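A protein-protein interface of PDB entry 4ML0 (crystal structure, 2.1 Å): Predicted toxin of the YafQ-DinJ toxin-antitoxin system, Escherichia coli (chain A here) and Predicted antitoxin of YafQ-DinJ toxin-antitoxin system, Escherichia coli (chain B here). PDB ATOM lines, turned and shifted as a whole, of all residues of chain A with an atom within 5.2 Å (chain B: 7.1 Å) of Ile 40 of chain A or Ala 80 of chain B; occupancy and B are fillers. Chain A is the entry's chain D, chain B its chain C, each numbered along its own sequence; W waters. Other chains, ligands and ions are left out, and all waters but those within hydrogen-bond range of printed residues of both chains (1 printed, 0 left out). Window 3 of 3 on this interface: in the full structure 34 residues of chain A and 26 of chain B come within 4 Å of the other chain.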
ATOM      1  N   GLN A   6     -27.421 -37.515 -13.363  1.00  0.00           N
ATOM      2  CA  GLN A   6     -27.530 -36.430 -12.393  1.00  0.00           C
ATOM      3  C   GLN A   6     -26.258 -35.591 -12.400  1.00  0.00           C
ATOM      4  O   GLN A   6     -25.150 -36.121 -12.553  1.00  0.00           O
ATOM      5  CB  GLN A   6     -27.780 -36.993 -10.995  1.00  0.00           C
ATOM      6  CG  GLN A   6     -28.849 -36.252 -10.205  1.00  0.00           C
ATOM      7  CD  GLN A   6     -29.299 -37.023  -8.970  1.00  0.00           C
ATOM      8  OE1 GLN A   6     -28.565 -37.867  -8.442  1.00  0.00           O
ATOM      9  NE2 GLN A   6     -30.515 -36.743  -8.511  1.00  0.00           N
ATOM     10  N   ILE A   9     -22.795 -31.534  -7.898  1.00  0.00           N
ATOM     11  CA  ILE A   9     -23.144 -30.236  -7.340  1.00  0.00           C
ATOM     12  C   ILE A   9     -21.962 -29.649  -6.587  1.00  0.00           C
ATOM     13  O   ILE A   9     -21.389 -30.312  -5.713  1.00  0.00           O
ATOM     14  CB  ILE A   9     -24.340 -30.355  -6.381  1.00  0.00           C
ATOM     15  CG1 ILE A   9     -25.549 -30.956  -7.108  1.00  0.00           C
ATOM     16  CG2 ILE A   9     -24.677 -29.007  -5.757  1.00  0.00           C
ATOM     17  CD1 ILE A   9     -26.686 -31.370  -6.182  1.00  0.00           C
ATOM     18  N   MET A  36     -32.534 -22.646  -7.106  1.00  0.00           N
ATOM     19  CA  MET A  36     -31.435 -23.617  -7.023  1.00  0.00           C
ATOM     20  C   MET A  36     -31.947 -25.057  -7.170  1.00  0.00           C
ATOM     21  O   MET A  36     -31.325 -25.883  -7.835  1.00  0.00           O
ATOM     22  CB  MET A  36     -30.654 -23.448  -5.706  1.00  0.00           C
ATOM     23  CG  MET A  36     -30.008 -22.053  -5.513  1.00  0.00           C
ATOM     24  SD  MET A  36     -29.237 -21.809  -3.882  1.00  0.00           S
ATOM     25  CE  MET A  36     -27.914 -23.025  -3.965  1.00  0.00           C
ATOM     26  N   THR A  37     -33.099 -25.329  -6.564  1.00  0.00           N
ATOM     27  CA  THR A  37     -33.729 -26.648  -6.643  1.00  0.00           C
ATOM     28  C   THR A  37     -34.134 -26.954  -8.085  1.00  0.00           C
ATOM     29  O   THR A  37     -33.916 -28.067  -8.579  1.00  0.00           O
ATOM     30  CB  THR A  37     -34.947 -26.737  -5.716  1.00  0.00           C
ATOM     31  OG1 THR A  37     -34.525 -26.513  -4.364  1.00  0.00           O
ATOM     32  CG2 THR A  37     -35.612 -28.112  -5.815  1.00  0.00           C
ATOM     33  N   LEU A  38     -34.700 -25.956  -8.762  1.00  0.00           N
ATOM     34  CA  LEU A  38     -34.979 -26.081 -10.193  1.00  0.00           C
ATOM     35  C   LEU A  38     -33.724 -26.502 -10.965  1.00  0.00           C
ATOM     36  O   LEU A  38     -33.780 -27.406 -11.814  1.00  0.00           O
ATOM     37  CB  LEU A  38     -35.518 -24.762 -10.756  1.00  0.00           C
ATOM     38  CG  LEU A  38     -37.013 -24.575 -11.007  1.00  0.00           C
ATOM     39  CD1 LEU A  38     -37.864 -25.279  -9.970  1.00  0.00           C
ATOM     40  CD2 LEU A  38     -37.354 -23.091 -11.038  1.00  0.00           C
ATOM     41  N   LEU A  39     -32.591 -25.858 -10.667  1.00  0.00           N
ATOM     42  CA  LEU A  39     -31.327 -26.178 -11.359  1.00  0.00           C
ATOM     43  C   LEU A  39     -30.809 -27.590 -11.062  1.00  0.00           C
ATOM     44  O   LEU A  39     -30.369 -28.324 -11.964  1.00  0.00           O
ATOM     45  CB  LEU A  39     -30.227 -25.178 -10.978  1.00  0.00           C
ATOM     46  CG  LEU A  39     -30.036 -23.845 -11.717  1.00  0.00           C
ATOM     47  CD1 LEU A  39     -30.581 -23.859 -13.142  1.00  0.00           C
ATOM     48  CD2 LEU A  39     -30.567 -22.650 -10.921  1.00  0.00           C
ATOM     49  N   ILE A  40     -30.830 -27.942  -9.780  1.00  0.00           N
ATOM     50  CA  ILE A  40     -30.358 -29.247  -9.321  1.00  0.00           C
ATOM     51  C   ILE A  40     -31.158 -30.388  -9.972  1.00  0.00           C
ATOM     52  O   ILE A  40     -30.579 -31.388 -10.402  1.00  0.00           O
ATOM     53  CB  ILE A  40     -30.428 -29.340  -7.782  1.00  0.00           C
ATOM     54  CG1 ILE A  40     -29.352 -28.445  -7.155  1.00  0.00           C
ATOM     55  CG2 ILE A  40     -30.246 -30.786  -7.314  1.00  0.00           C
ATOM     56  CD1 ILE A  40     -29.567 -28.118  -5.680  1.00  0.00           C
ATOM     57  N   ASN A  41     -32.477 -30.217 -10.068  1.00  0.00           N
ATOM     58  CA  ASN A  41     -33.353 -31.259 -10.620  1.00  0.00           C
ATOM     59  C   ASN A  41     -33.422 -31.275 -12.139  1.00  0.00           C
ATOM     60  O   ASN A  41     -34.231 -32.012 -12.717  1.00  0.00           O
ATOM     61  CB  ASN A  41     -34.771 -31.145 -10.048  1.00  0.00           C
ATOM     62  CG  ASN A  41     -34.818 -31.418  -8.561  1.00  0.00           C
ATOM     63  OD1 ASN A  41     -33.895 -32.016  -7.997  1.00  0.00           O
ATOM     64  ND2 ASN A  41     -35.893 -30.977  -7.910  1.00  0.00           N
ATOM     65  N   ASN A  42     -32.577 -30.462 -12.774  1.00  0.00           N
ATOM     66  CA  ASN A  42     -32.576 -30.302 -14.231  1.00  0.00           C
ATOM     67  C   ASN A  42     -33.969 -29.991 -14.778  1.00  0.00           C
ATOM     68  O   ASN A  42     -34.303 -30.368 -15.899  1.00  0.00           O
ATOM     69  CB  ASN A  42     -31.981 -31.532 -14.937  1.00  0.00           C
ATOM     70  CG  ASN A  42     -31.601 -31.252 -16.391  1.00  0.00           C
ATOM     71  OD1 ASN A  42     -31.004 -30.218 -16.701  1.00  0.00           O
ATOM     72  ND2 ASN A  42     -31.967 -32.163 -17.288  1.00  0.00           N
ATOM     73  N   LEU A  82     -22.862 -28.731 -11.992  1.00  0.00           N
ATOM     74  CA  LEU A  82     -23.604 -27.518 -11.701  1.00  0.00           C
ATOM     75  C   LEU A  82     -22.939 -26.836 -10.490  1.00  0.00           C
ATOM     76  O   LEU A  82     -23.027 -27.334  -9.360  1.00  0.00           O
ATOM     77  CB  LEU A  82     -25.056 -27.891 -11.437  1.00  0.00           C
ATOM     78  CG  LEU A  82     -26.141 -26.881 -11.063  1.00  0.00           C
ATOM     79  CD1 LEU A  82     -26.237 -26.823  -9.578  1.00  0.00           C
ATOM     80  CD2 LEU A  82     -25.895 -25.484 -11.647  1.00  0.00           C
ATOM     81  N   PHE A  84     -22.666 -23.486  -8.092  1.00  0.00           N
ATOM     82  CA  PHE A  84     -23.184 -22.190  -7.663  1.00  0.00           C
ATOM     83  C   PHE A  84     -22.018 -21.243  -7.378  1.00  0.00           C
ATOM     84  O   PHE A  84     -21.187 -21.506  -6.497  1.00  0.00           O
ATOM     85  CB  PHE A  84     -24.121 -22.352  -6.456  1.00  0.00           C
ATOM     86  CG  PHE A  84     -25.375 -23.134  -6.776  1.00  0.00           C
ATOM     87  CD1 PHE A  84     -26.387 -22.564  -7.546  1.00  0.00           C
ATOM     88  CD2 PHE A  84     -25.528 -24.449  -6.335  1.00  0.00           C
ATOM     89  CE1 PHE A  84     -27.542 -23.284  -7.862  1.00  0.00           C
ATOM     90  CE2 PHE A  84     -26.680 -25.176  -6.639  1.00  0.00           C
ATOM     91  CZ  PHE A  84     -27.691 -24.591  -7.410  1.00  0.00           C
ATOM     92  N   ALA B  77     -21.488 -30.888  -2.637  1.00  0.00           N
ATOM     93  CA  ALA B  77     -22.738 -31.202  -1.955  1.00  0.00           C
ATOM     94  C   ALA B  77     -23.327 -32.422  -2.642  1.00  0.00           C
ATOM     95  O   ALA B  77     -23.156 -32.598  -3.849  1.00  0.00           O
ATOM     96  CB  ALA B  77     -23.698 -30.034  -2.001  1.00  0.00           C
ATOM     97  N   LYS B  78     -24.007 -33.267  -1.877  1.00  0.00           N
ATOM     98  CA  LYS B  78     -24.507 -34.531  -2.408  1.00  0.00           C
ATOM     99  C   LYS B  78     -25.895 -34.354  -3.010  1.00  0.00           C
ATOM    100  O   LYS B  78     -26.233 -34.973  -4.020  1.00  0.00           O
ATOM    101  CB  LYS B  78     -24.517 -35.586  -1.304  1.00  0.00           C
ATOM    102  CG  LYS B  78     -23.185 -35.665  -0.567  1.00  0.00           C
ATOM    103  CD  LYS B  78     -23.339 -36.171   0.863  1.00  0.00           C
ATOM    104  CE  LYS B  78     -22.236 -35.604   1.756  1.00  0.00           C
ATOM    105  NZ  LYS B  78     -20.873 -35.805   1.178  1.00  0.00           N
ATOM    106  N   ASP B  79     -26.687 -33.490  -2.386  1.00  0.00           N
ATOM    107  CA  ASP B  79     -28.027 -33.176  -2.861  1.00  0.00           C
ATOM    108  C   ASP B  79     -28.464 -31.816  -2.323  1.00  0.00           C
ATOM    109  O   ASP B  79     -27.729 -31.182  -1.559  1.00  0.00           O
ATOM    110  CB  ASP B  79     -29.018 -34.263  -2.432  1.00  0.00           C
ATOM    111  CG  ASP B  79     -28.931 -34.589  -0.944  1.00  0.00           C
ATOM    112  OD1 ASP B  79     -28.825 -33.655  -0.114  1.00  0.00           O
ATOM    113  OD2 ASP B  79     -28.973 -35.793  -0.608  1.00  0.00           O
ATOM    114  N   ALA B  80     -29.660 -31.377  -2.711  1.00  0.00           N
ATOM    115  CA  ALA B  80     -30.179 -30.071  -2.306  1.00  0.00           C
ATOM    116  C   ALA B  80     -30.251 -29.878  -0.786  1.00  0.00           C
ATOM    117  O   ALA B  80     -29.958 -28.792  -0.281  1.00  0.00           O
ATOM    118  CB  ALA B  80     -31.546 -29.810  -2.952  1.00  0.00           C
ATOM    119  N   ASP B  81     -30.651 -30.923  -0.064  1.00  0.00           N
ATOM    120  CA  ASP B  81     -30.711 -30.866   1.398  1.00  0.00           C
ATOM    121  C   ASP B  81     -29.327 -30.640   2.012  1.00  0.00           C
ATOM    122  O   ASP B  81     -29.150 -29.772   2.881  1.00  0.00           O
ATOM    123  CB  ASP B  81     -31.333 -32.151   1.960  1.00  0.00           C
ATOM    124  CG  ASP B  81     -32.848 -32.195   1.799  1.00  0.00           C
ATOM    125  OD1 ASP B  81     -33.485 -33.070   2.427  1.00  0.00           O
ATOM    126  OD2 ASP B  81     -33.401 -31.353   1.056  1.00  0.00           O
ATOM    127  N   ASP B  82     -28.355 -31.427   1.552  1.00  0.00           N
ATOM    128  CA  ASP B  82     -26.967 -31.306   1.990  1.00  0.00           C
ATOM    129  C   ASP B  82     -26.446 -29.894   1.707  1.00  0.00           C
ATOM    130  O   ASP B  82     -25.835 -29.248   2.570  1.00  0.00           O
ATOM    131  CB  ASP B  82     -26.096 -32.339   1.257  1.00  0.00           C
ATOM    132  CG  ASP B  82     -24.646 -32.331   1.728  1.00  0.00           C
ATOM    133  OD1 ASP B  82     -24.424 -32.220   2.955  1.00  0.00           O
ATOM    134  OD2 ASP B  82     -23.728 -32.439   0.879  1.00  0.00           O
ATOM    135  N   LEU B  83     -26.706 -29.421   0.490  1.00  0.00           N
ATOM    136  CA  LEU B  83     -26.284 -28.090   0.067  1.00  0.00           C
ATOM    137  C   LEU B  83     -26.853 -27.003   0.973  1.00  0.00           C
ATOM    138  O   LEU B  83     -26.110 -26.185   1.524  1.00  0.00           O
ATOM    139  CB  LEU B  83     -26.709 -27.844  -1.382  1.00  0.00           C
ATOM    140  CG  LEU B  83     -26.450 -26.454  -1.961  1.00  0.00           C
ATOM    141  CD1 LEU B  83     -24.981 -26.094  -1.866  1.00  0.00           C
ATOM    142  CD2 LEU B  83     -26.894 -26.421  -3.406  1.00  0.00           C
ATOM    143  N   PHE B  84     -28.174 -27.003   1.125  1.00  0.00           N
ATOM    144  CA  PHE B  84     -28.863 -25.996   1.927  1.00  0.00           C
ATOM    145  C   PHE B  84     -28.395 -26.004   3.379  1.00  0.00           C
ATOM    146  O   PHE B  84     -28.278 -24.941   4.006  1.00  0.00           O
ATOM    147  CB  PHE B  84     -30.381 -26.198   1.861  1.00  0.00           C
ATOM    148  CG  PHE B  84     -30.965 -25.969   0.495  1.00  0.00           C
ATOM    149  CD1 PHE B  84     -30.294 -25.186  -0.443  1.00  0.00           C
ATOM    150  CD2 PHE B  84     -32.187 -26.531   0.147  1.00  0.00           C
ATOM    151  CE1 PHE B  84     -30.833 -24.967  -1.709  1.00  0.00           C
ATOM    152  CE2 PHE B  84     -32.733 -26.320  -1.117  1.00  0.00           C
ATOM    153  CZ  PHE B  84     -32.053 -25.538  -2.048  1.00  0.00           C
ATOM    154  N   ASP B  85     -28.131 -27.198   3.914  1.00  0.00           N
ATOM    155  CA  ASP B  85     -27.588 -27.297   5.267  1.00  0.00           C
ATOM    156  C   ASP B  85     -26.187 -26.671   5.339  1.00  0.00           C
ATOM    157  O   ASP B  85     -25.900 -25.864   6.229  1.00  0.00           O
ATOM    158  CB  ASP B  85     -27.574 -28.753   5.764  1.00  0.00           C
ATOM    159  CG  ASP B  85     -27.040 -28.884   7.194  1.00  0.00           C
ATOM    160  OD1 ASP B  85     -27.794 -28.574   8.150  1.00  0.00           O
ATOM    161  OD2 ASP B  85     -25.866 -29.298   7.361  1.00  0.00           O
ATOM    162  N   LYS B  86     -25.328 -27.031   4.388  1.00  0.00           N
ATOM    163  CA  LYS B  86     -23.975 -26.489   4.343  1.00  0.00           C
ATOM    164  C   LYS B  86     -23.933 -24.965   4.189  1.00  0.00           C
ATOM    165  O   LYS B  86     -23.022 -24.319   4.699  1.00  0.00           O
ATOM    166  CB  LYS B  86     -23.161 -27.171   3.241  1.00  0.00           C
ATOM    167  CG  LYS B  86     -22.687 -28.566   3.618  1.00  0.00           C
ATOM    168  CD  LYS B  86     -22.354 -29.428   2.399  1.00  0.00           C
ATOM    169  CE  LYS B  86     -21.536 -30.652   2.818  1.00  0.00           C
ATOM    170  NZ  LYS B  86     -21.249 -31.620   1.706  1.00  0.00           N
ATOM    171  N   ILE B  89     -29.057 -22.330   5.032  1.00  0.00           N
ATOM    172  CA  ILE B  89     -30.350 -21.773   4.621  1.00  0.00           C
ATOM    173  C   ILE B  89     -31.434 -22.845   4.510  1.00  0.00           C
ATOM    174  O   ILE B  89     -31.139 -24.037   4.405  1.00  0.00           O
ATOM    175  CB  ILE B  89     -30.261 -21.001   3.278  1.00  0.00           C
ATOM    176  CG1 ILE B  89     -29.882 -21.940   2.128  1.00  0.00           C
ATOM    177  CG2 ILE B  89     -29.274 -19.853   3.389  1.00  0.00           C
ATOM    178  CD1 ILE B  89     -29.703 -21.232   0.779  1.00  0.00           C
HETATM  179  O   HOH W   1     -23.432 -33.892  -6.140  1.00  0.00           O
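The backbone NH of Ala 77 of chain B lies within hydrogen-bond range of the backbone carbonyl oxygen of Ile 9 of chain A.
O of Phe 84 of chain B lies within hydrogen-bond range of N of Ile 89 of chain B, at 2.9 Å.
Leu 83 of chain B touches Met 36 of chain A. Thr 37 of chain A touches Phe 84 of chain B (OG1 to CZ, 3.5 Å). Ile 40 of chain A touches Ala 80 of chain B. Ile 40 of chain A touches Leu 83 of chain B (CD1 to CD2, 3.9 Å). Phe 84 of chain A touches Leu 83 of chain B.
Of the printed residues of chain B, Ile 9 of chain A touches Ala 77. Printed residues of chain B within 4 Å of Met 36 of chain A: Leu 83 (3.6 Å). Leu 38 of chain A touches none of the printed residues of chain B. Ile 40 of chain A touches two residues of chain B. Of the printed residues of chain B, Phe 84 of chain A touches Leu 83 (3.5 Å). Of the printed residues of chain A, Ala 77 of chain B touches Ile 9 (3.1 Å). Of chain A, only Ile 40 (3.8 Å) comes within 4 Å of Ala 80 of chain B. Printed residues of chain A within 4 Å of Phe 84 of chain B: Thr 37 (3.5 Å). The nearest residue of chain A that does not touch Ala 80 of chain B is Ile 9 of chain A (4.6 Å). The nearest printed residue of chain A that does not touch Leu 83 of chain B is Ile 9 of chain A (4.1 Å).
Printed residues of chain A that touch a printed residue of chain B: Ile 9, Met 36, Thr 37, Ile 40 and Phe 84. Hydrophobic or aromatic side chains of chain A within 4 Å of the printed part of chain B: Ile 9, Met 36, Ile 40 and Phe 84. Hydrophobic or aromatic side chains of chain B that line the printed part of chain A: Ala 80, Leu 83 and Phe 84. Along chain B the printed residues that touch a printed residue of chain A span positions 77 to 84.
Water W1 lies within hydrogen-bond range of the backbone carbonyl oxygen (O) of Ala 77 of chain B (2.6 Å) and the backbone NH (N) of Ile 9 of chain A (3.0 Å).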
